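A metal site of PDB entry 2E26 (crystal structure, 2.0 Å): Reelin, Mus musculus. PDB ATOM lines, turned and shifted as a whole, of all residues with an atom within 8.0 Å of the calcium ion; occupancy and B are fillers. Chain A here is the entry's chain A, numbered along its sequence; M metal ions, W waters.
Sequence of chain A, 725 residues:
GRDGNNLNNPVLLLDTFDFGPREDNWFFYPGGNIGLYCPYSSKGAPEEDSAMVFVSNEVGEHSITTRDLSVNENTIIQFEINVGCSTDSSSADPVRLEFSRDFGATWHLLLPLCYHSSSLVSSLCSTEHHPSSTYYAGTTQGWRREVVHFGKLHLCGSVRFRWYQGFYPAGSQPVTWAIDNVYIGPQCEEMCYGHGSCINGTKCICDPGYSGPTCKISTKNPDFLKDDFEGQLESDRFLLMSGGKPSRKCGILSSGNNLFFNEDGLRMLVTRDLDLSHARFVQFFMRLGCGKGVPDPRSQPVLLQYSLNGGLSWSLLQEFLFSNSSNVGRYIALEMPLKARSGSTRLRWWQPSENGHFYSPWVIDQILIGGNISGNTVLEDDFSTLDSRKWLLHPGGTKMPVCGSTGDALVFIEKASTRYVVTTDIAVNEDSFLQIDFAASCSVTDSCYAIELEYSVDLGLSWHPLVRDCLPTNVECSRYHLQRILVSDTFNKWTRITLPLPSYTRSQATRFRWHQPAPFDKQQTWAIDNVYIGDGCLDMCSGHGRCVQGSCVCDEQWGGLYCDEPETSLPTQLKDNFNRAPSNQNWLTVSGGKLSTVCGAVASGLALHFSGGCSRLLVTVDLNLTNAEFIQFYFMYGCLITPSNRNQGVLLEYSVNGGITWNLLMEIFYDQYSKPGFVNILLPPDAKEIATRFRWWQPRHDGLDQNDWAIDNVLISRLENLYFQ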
ATOM      1  N   ASP A 576     -28.447 -16.535  -7.629  1.00  0.00           N
ATOM      2  CA  ASP A 576     -29.193 -15.452  -6.996  1.00  0.00           C
ATOM      3  C   ASP A 576     -28.589 -14.093  -7.354  1.00  0.00           C
ATOM      4  O   ASP A 576     -27.424 -13.827  -7.041  1.00  0.00           O
ATOM      5  CB  ASP A 576     -29.210 -15.632  -5.476  1.00  0.00           C
ATOM      6  CG  ASP A 576     -30.432 -14.982  -4.823  1.00  0.00           C
ATOM      7  OD1 ASP A 576     -30.930 -13.970  -5.357  1.00  0.00           O
ATOM      8  OD2 ASP A 576     -30.877 -15.495  -3.767  1.00  0.00           O
ATOM      9  N   ASN A 577     -29.392 -13.249  -8.010  1.00  0.00           N
ATOM     10  CA  ASN A 577     -29.008 -11.871  -8.332  1.00  0.00           C
ATOM     11  C   ASN A 577     -29.389 -10.867  -7.240  1.00  0.00           C
ATOM     12  O   ASN A 577     -29.131  -9.668  -7.360  1.00  0.00           O
ATOM     13  CB  ASN A 577     -29.582 -11.427  -9.698  1.00  0.00           C
ATOM     14  CG  ASN A 577     -31.121 -11.477  -9.762  1.00  0.00           C
ATOM     15  OD1 ASN A 577     -31.694 -11.273 -10.841  1.00  0.00           O
ATOM     16  ND2 ASN A 577     -31.784 -11.718  -8.638  1.00  0.00           N
ATOM     17  N   PHE A 578     -30.015 -11.379  -6.187  1.00  0.00           N
ATOM     18  CA  PHE A 578     -30.394 -10.588  -4.998  1.00  0.00           C
ATOM     19  C   PHE A 578     -31.215  -9.351  -5.316  1.00  0.00           C
ATOM     20  O   PHE A 578     -31.072  -8.323  -4.657  1.00  0.00           O
ATOM     21  CB  PHE A 578     -29.158 -10.187  -4.199  1.00  0.00           C
ATOM     22  CG  PHE A 578     -28.360 -11.339  -3.671  1.00  0.00           C
ATOM     23  CD1 PHE A 578     -28.846 -12.102  -2.612  1.00  0.00           C
ATOM     24  CD2 PHE A 578     -27.131 -11.653  -4.226  1.00  0.00           C
ATOM     25  CE1 PHE A 578     -28.101 -13.171  -2.113  1.00  0.00           C
ATOM     26  CE2 PHE A 578     -26.396 -12.717  -3.756  1.00  0.00           C
ATOM     27  CZ  PHE A 578     -26.872 -13.483  -2.682  1.00  0.00           C
ATOM     28  N   ASN A 579     -32.064  -9.444  -6.347  1.00  0.00           N
ATOM     29  CA  ASN A 579     -32.968  -8.362  -6.688  1.00  0.00           C
ATOM     30  C   ASN A 579     -34.359  -8.551  -6.070  1.00  0.00           C
ATOM     31  O   ASN A 579     -35.220  -7.664  -6.158  1.00  0.00           O
ATOM     32  CB  ASN A 579     -33.042  -8.189  -8.210  1.00  0.00           C
ATOM     33  CG  ASN A 579     -31.662  -7.888  -8.843  1.00  0.00           C
ATOM     34  OD1 ASN A 579     -30.770  -7.281  -8.228  1.00  0.00           O
ATOM     35  ND2 ASN A 579     -31.503  -8.303 -10.097  1.00  0.00           N
ATOM     36  N   ARG A 580     -34.565  -9.705  -5.437  1.00  0.00           N
ATOM     37  CA  ARG A 580     -35.742  -9.978  -4.615  1.00  0.00           C
ATOM     38  C   ARG A 580     -35.301 -10.565  -3.278  1.00  0.00           C
ATOM     39  O   ARG A 580     -34.202 -11.107  -3.173  1.00  0.00           O
ATOM     40  CB  ARG A 580     -36.701 -10.918  -5.351  1.00  0.00           C
ATOM     41  CG  ARG A 580     -37.575 -10.213  -6.394  1.00  0.00           C
ATOM     42  CD  ARG A 580     -37.958 -11.117  -7.573  1.00  0.00           C
ATOM     43  NE  ARG A 580     -36.831 -11.351  -8.482  1.00  0.00           N
ATOM     44  CZ  ARG A 580     -36.627 -10.719  -9.642  1.00  0.00           C
ATOM     45  NH1 ARG A 580     -37.464  -9.797 -10.083  1.00  0.00           N
ATOM     46  NH2 ARG A 580     -35.558 -11.031 -10.372  1.00  0.00           N
ATOM     47  N   LEU A 595     -31.036  -6.649   1.621  1.00  0.00           N
ATOM     48  CA  LEU A 595     -30.865  -6.064   0.300  1.00  0.00           C
ATOM     49  C   LEU A 595     -30.792  -4.551   0.437  1.00  0.00           C
ATOM     50  O   LEU A 595     -31.608  -3.968   1.149  1.00  0.00           O
ATOM     51  CB  LEU A 595     -32.029  -6.450  -0.610  1.00  0.00           C
ATOM     52  CG  LEU A 595     -32.320  -7.930  -0.866  1.00  0.00           C
ATOM     53  CD1 LEU A 595     -33.382  -8.048  -1.941  1.00  0.00           C
ATOM     54  CD2 LEU A 595     -31.048  -8.702  -1.267  1.00  0.00           C
ATOM     55  N   SER A 596     -29.807  -3.929  -0.202  1.00  0.00           N
ATOM     56  CA  SER A 596     -29.757  -2.465  -0.298  1.00  0.00           C
ATOM     57  C   SER A 596     -29.001  -1.946  -1.520  1.00  0.00           C
ATOM     58  O   SER A 596     -28.411  -2.720  -2.271  1.00  0.00           O
ATOM     59  CB  SER A 596     -29.226  -1.832   1.000  1.00  0.00           C
ATOM     60  OG  SER A 596     -27.824  -1.857   1.062  1.00  0.00           O
ATOM     61  N   GLY A 600     -23.743   0.960  -3.895  1.00  0.00           N
ATOM     62  CA  GLY A 600     -23.770   1.208  -5.339  1.00  0.00           C
ATOM     63  C   GLY A 600     -23.969  -0.132  -6.035  1.00  0.00           C
ATOM     64  O   GLY A 600     -24.460  -1.102  -5.416  1.00  0.00           O
ATOM     65  N   ALA A 601     -23.591  -0.201  -7.307  1.00  0.00           N
ATOM     66  CA  ALA A 601     -23.624  -1.481  -8.018  1.00  0.00           C
ATOM     67  C   ALA A 601     -22.442  -2.353  -7.605  1.00  0.00           C
ATOM     68  O   ALA A 601     -21.286  -1.963  -7.766  1.00  0.00           O
ATOM     69  CB  ALA A 601     -23.613  -1.253  -9.522  1.00  0.00           C
ATOM     70  N   VAL A 602     -22.749  -3.520  -7.056  1.00  0.00           N
ATOM     71  CA  VAL A 602     -21.750  -4.544  -6.760  1.00  0.00           C
ATOM     72  C   VAL A 602     -21.659  -5.423  -8.007  1.00  0.00           C
ATOM     73  O   VAL A 602     -20.586  -5.567  -8.598  1.00  0.00           O
ATOM     74  CB  VAL A 602     -22.119  -5.358  -5.514  1.00  0.00           C
ATOM     75  CG1 VAL A 602     -21.053  -6.421  -5.232  1.00  0.00           C
ATOM     76  CG2 VAL A 602     -22.297  -4.441  -4.313  1.00  0.00           C
ATOM     77  N   ALA A 603     -22.799  -5.998  -8.412  1.00  0.00           N
ATOM     78  CA  ALA A 603     -22.985  -6.457  -9.787  1.00  0.00           C
ATOM     79  C   ALA A 603     -23.979  -5.500 -10.425  1.00  0.00           C
ATOM     80  O   ALA A 603     -23.609  -4.677 -11.253  1.00  0.00           O
ATOM     81  CB  ALA A 603     -23.493  -7.891  -9.844  1.00  0.00           C
ATOM     82  N   SER A 604     -25.239  -5.569 -10.006  1.00  0.00           N
ATOM     83  CA  SER A 604     -26.245  -4.619 -10.445  1.00  0.00           C
ATOM     84  C   SER A 604     -27.406  -4.568  -9.470  1.00  0.00           C
ATOM     85  O   SER A 604     -27.708  -5.547  -8.770  1.00  0.00           O
ATOM     86  CB  SER A 604     -26.752  -4.968 -11.841  1.00  0.00           C
ATOM     87  OG  SER A 604     -27.359  -6.246 -11.842  1.00  0.00           O
ATOM     88  N   GLY A 605     -28.075  -3.425  -9.428  1.00  0.00           N
ATOM     89  CA  GLY A 605     -29.244  -3.220  -8.583  1.00  0.00           C
ATOM     90  C   GLY A 605     -28.916  -3.481  -7.123  1.00  0.00           C
ATOM     91  O   GLY A 605     -27.859  -3.062  -6.618  1.00  0.00           O
ATOM     92  N   LEU A 606     -29.827  -4.174  -6.453  1.00  0.00           N
ATOM     93  CA  LEU A 606     -29.676  -4.505  -5.045  1.00  0.00           C
ATOM     94  C   LEU A 606     -28.565  -5.517  -4.824  1.00  0.00           C
ATOM     95  O   LEU A 606     -28.312  -6.374  -5.682  1.00  0.00           O
ATOM     96  CB  LEU A 606     -31.005  -5.042  -4.483  1.00  0.00           C
ATOM     97  CG  LEU A 606     -32.213  -4.112  -4.497  1.00  0.00           C
ATOM     98  CD1 LEU A 606     -33.501  -4.887  -4.222  1.00  0.00           C
ATOM     99  CD2 LEU A 606     -32.050  -2.953  -3.504  1.00  0.00           C
ATOM    100  N   ALA A 607     -27.883  -5.384  -3.702  1.00  0.00           N
ATOM    101  CA  ALA A 607     -26.933  -6.390  -3.246  1.00  0.00           C
ATOM    102  C   ALA A 607     -27.360  -6.802  -1.848  1.00  0.00           C
ATOM    103  O   ALA A 607     -28.052  -6.043  -1.166  1.00  0.00           O
ATOM    104  CB  ALA A 607     -25.541  -5.810  -3.210  1.00  0.00           C
ATOM    105  N   LEU A 608     -26.978  -8.005  -1.445  1.00  0.00           N
ATOM    106  CA  LEU A 608     -27.216  -8.433  -0.082  1.00  0.00           C
ATOM    107  C   LEU A 608     -26.096  -7.858   0.798  1.00  0.00           C
ATOM    108  O   LEU A 608     -24.950  -8.314   0.733  1.00  0.00           O
ATOM    109  CB  LEU A 608     -27.261  -9.964   0.023  1.00  0.00           C
ATOM    110  CG  LEU A 608     -27.638 -10.500   1.407  1.00  0.00           C
ATOM    111  CD1 LEU A 608     -28.955  -9.913   1.889  1.00  0.00           C
ATOM    112  CD2 LEU A 608     -27.751 -12.008   1.379  1.00  0.00           C
ATOM    113  N   ILE A 711     -22.595  -8.876  -1.086  1.00  0.00           N
ATOM    114  CA  ILE A 711     -22.436  -9.905  -2.100  1.00  0.00           C
ATOM    115  C   ILE A 711     -23.502  -9.706  -3.174  1.00  0.00           C
ATOM    116  O   ILE A 711     -24.585  -9.207  -2.899  1.00  0.00           O
ATOM    117  CB  ILE A 711     -22.454 -11.342  -1.466  1.00  0.00           C
ATOM    118  CG1 ILE A 711     -22.039 -12.412  -2.491  1.00  0.00           C
ATOM    119  CG2 ILE A 711     -23.785 -11.649  -0.783  1.00  0.00           C
ATOM    120  CD1 ILE A 711     -21.617 -13.751  -1.875  1.00  0.00           C
ATOM    121  N   ASP A 712     -23.180 -10.087  -4.411  1.00  0.00           N
ATOM    122  CA  ASP A 712     -24.153  -9.989  -5.481  1.00  0.00           C
ATOM    123  C   ASP A 712     -23.879 -11.076  -6.511  1.00  0.00           C
ATOM    124  O   ASP A 712     -22.770 -11.618  -6.563  1.00  0.00           O
ATOM    125  CB  ASP A 712     -24.088  -8.587  -6.106  1.00  0.00           C
ATOM    126  CG  ASP A 712     -25.408  -8.174  -6.742  1.00  0.00           C
ATOM    127  OD1 ASP A 712     -26.375  -8.960  -6.709  1.00  0.00           O
ATOM    128  OD2 ASP A 712     -25.474  -7.032  -7.266  1.00  0.00           O
ATOM    129  N   ASN A 713     -24.909 -11.417  -7.288  1.00  0.00           N
ATOM    130  CA  ASN A 713     -24.837 -12.391  -8.373  1.00  0.00           C
ATOM    131  C   ASN A 713     -24.005 -13.629  -8.055  1.00  0.00           C
ATOM    132  O   ASN A 713     -22.950 -13.863  -8.655  1.00  0.00           O
ATOM    133  CB  ASN A 713     -24.390 -11.742  -9.691  1.00  0.00           C
ATOM    134  CG  ASN A 713     -25.472 -10.875 -10.312  1.00  0.00           C
ATOM    135  OD1 ASN A 713     -26.357 -10.395  -9.598  1.00  0.00           O
ATOM    136  ND2 ASN A 713     -25.413 -10.671 -11.632  1.00  0.00           N
ATOM    137  N   VAL A 714     -24.501 -14.398  -7.076  1.00  0.00           N
ATOM    138  CA  VAL A 714     -23.957 -15.712  -6.726  1.00  0.00           C
ATOM    139  C   VAL A 714     -24.367 -16.696  -7.813  1.00  0.00           C
ATOM    140  O   VAL A 714     -25.521 -16.708  -8.252  1.00  0.00           O
ATOM    141  CB  VAL A 714     -24.522 -16.219  -5.377  1.00  0.00           C
ATOM    142  CG1 VAL A 714     -23.902 -17.583  -4.985  1.00  0.00           C
ATOM    143  CG2 VAL A 714     -24.252 -15.218  -4.281  1.00  0.00           C
HETATM  144 CA    CA M   1     -28.177  -7.582  -7.629  1.00  0.00          CA
HETATM  145  O   HOH W   1     -27.753  -8.330 -10.003  1.00  0.00           O
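N of Ala 603 lies close to OD2 of Asp 712 (3.1 Å). N of Asn 713 sits close to O of Asp 576 (3.5 Å). The side-chain amide oxygen (OD1) of Asn 713 lies close to the side-chain carboxylate (OD1) of Asp 712, at 3.2 Å.
Asn 713 touches the calcium ion (OD1 to CA, 3.9 Å). Of the 20 residues printed, 6 come within 4 Å of the calcium ion. The nearest printed residue that does not touch the calcium ion is Gly 605 (4.2 Å).
The calcium ion is bound by O of Leu 606 (2.3 Å), O of Asn 577 (2.3 Å), O of Ser 604 (2.4 Å), OD1 of Asp 712 (2.4 Å), water W1 (2.5 Å), OD1 of Asn 579 (2.7 Å) and OD2 of Asp 712 (2.8 Å).
Water W1 bridges the side-chain amide oxygen (OD1) of Asn 713 (2.5 Å) and the side-chain hydroxyl (OG) of Ser 604 (2.8 Å).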
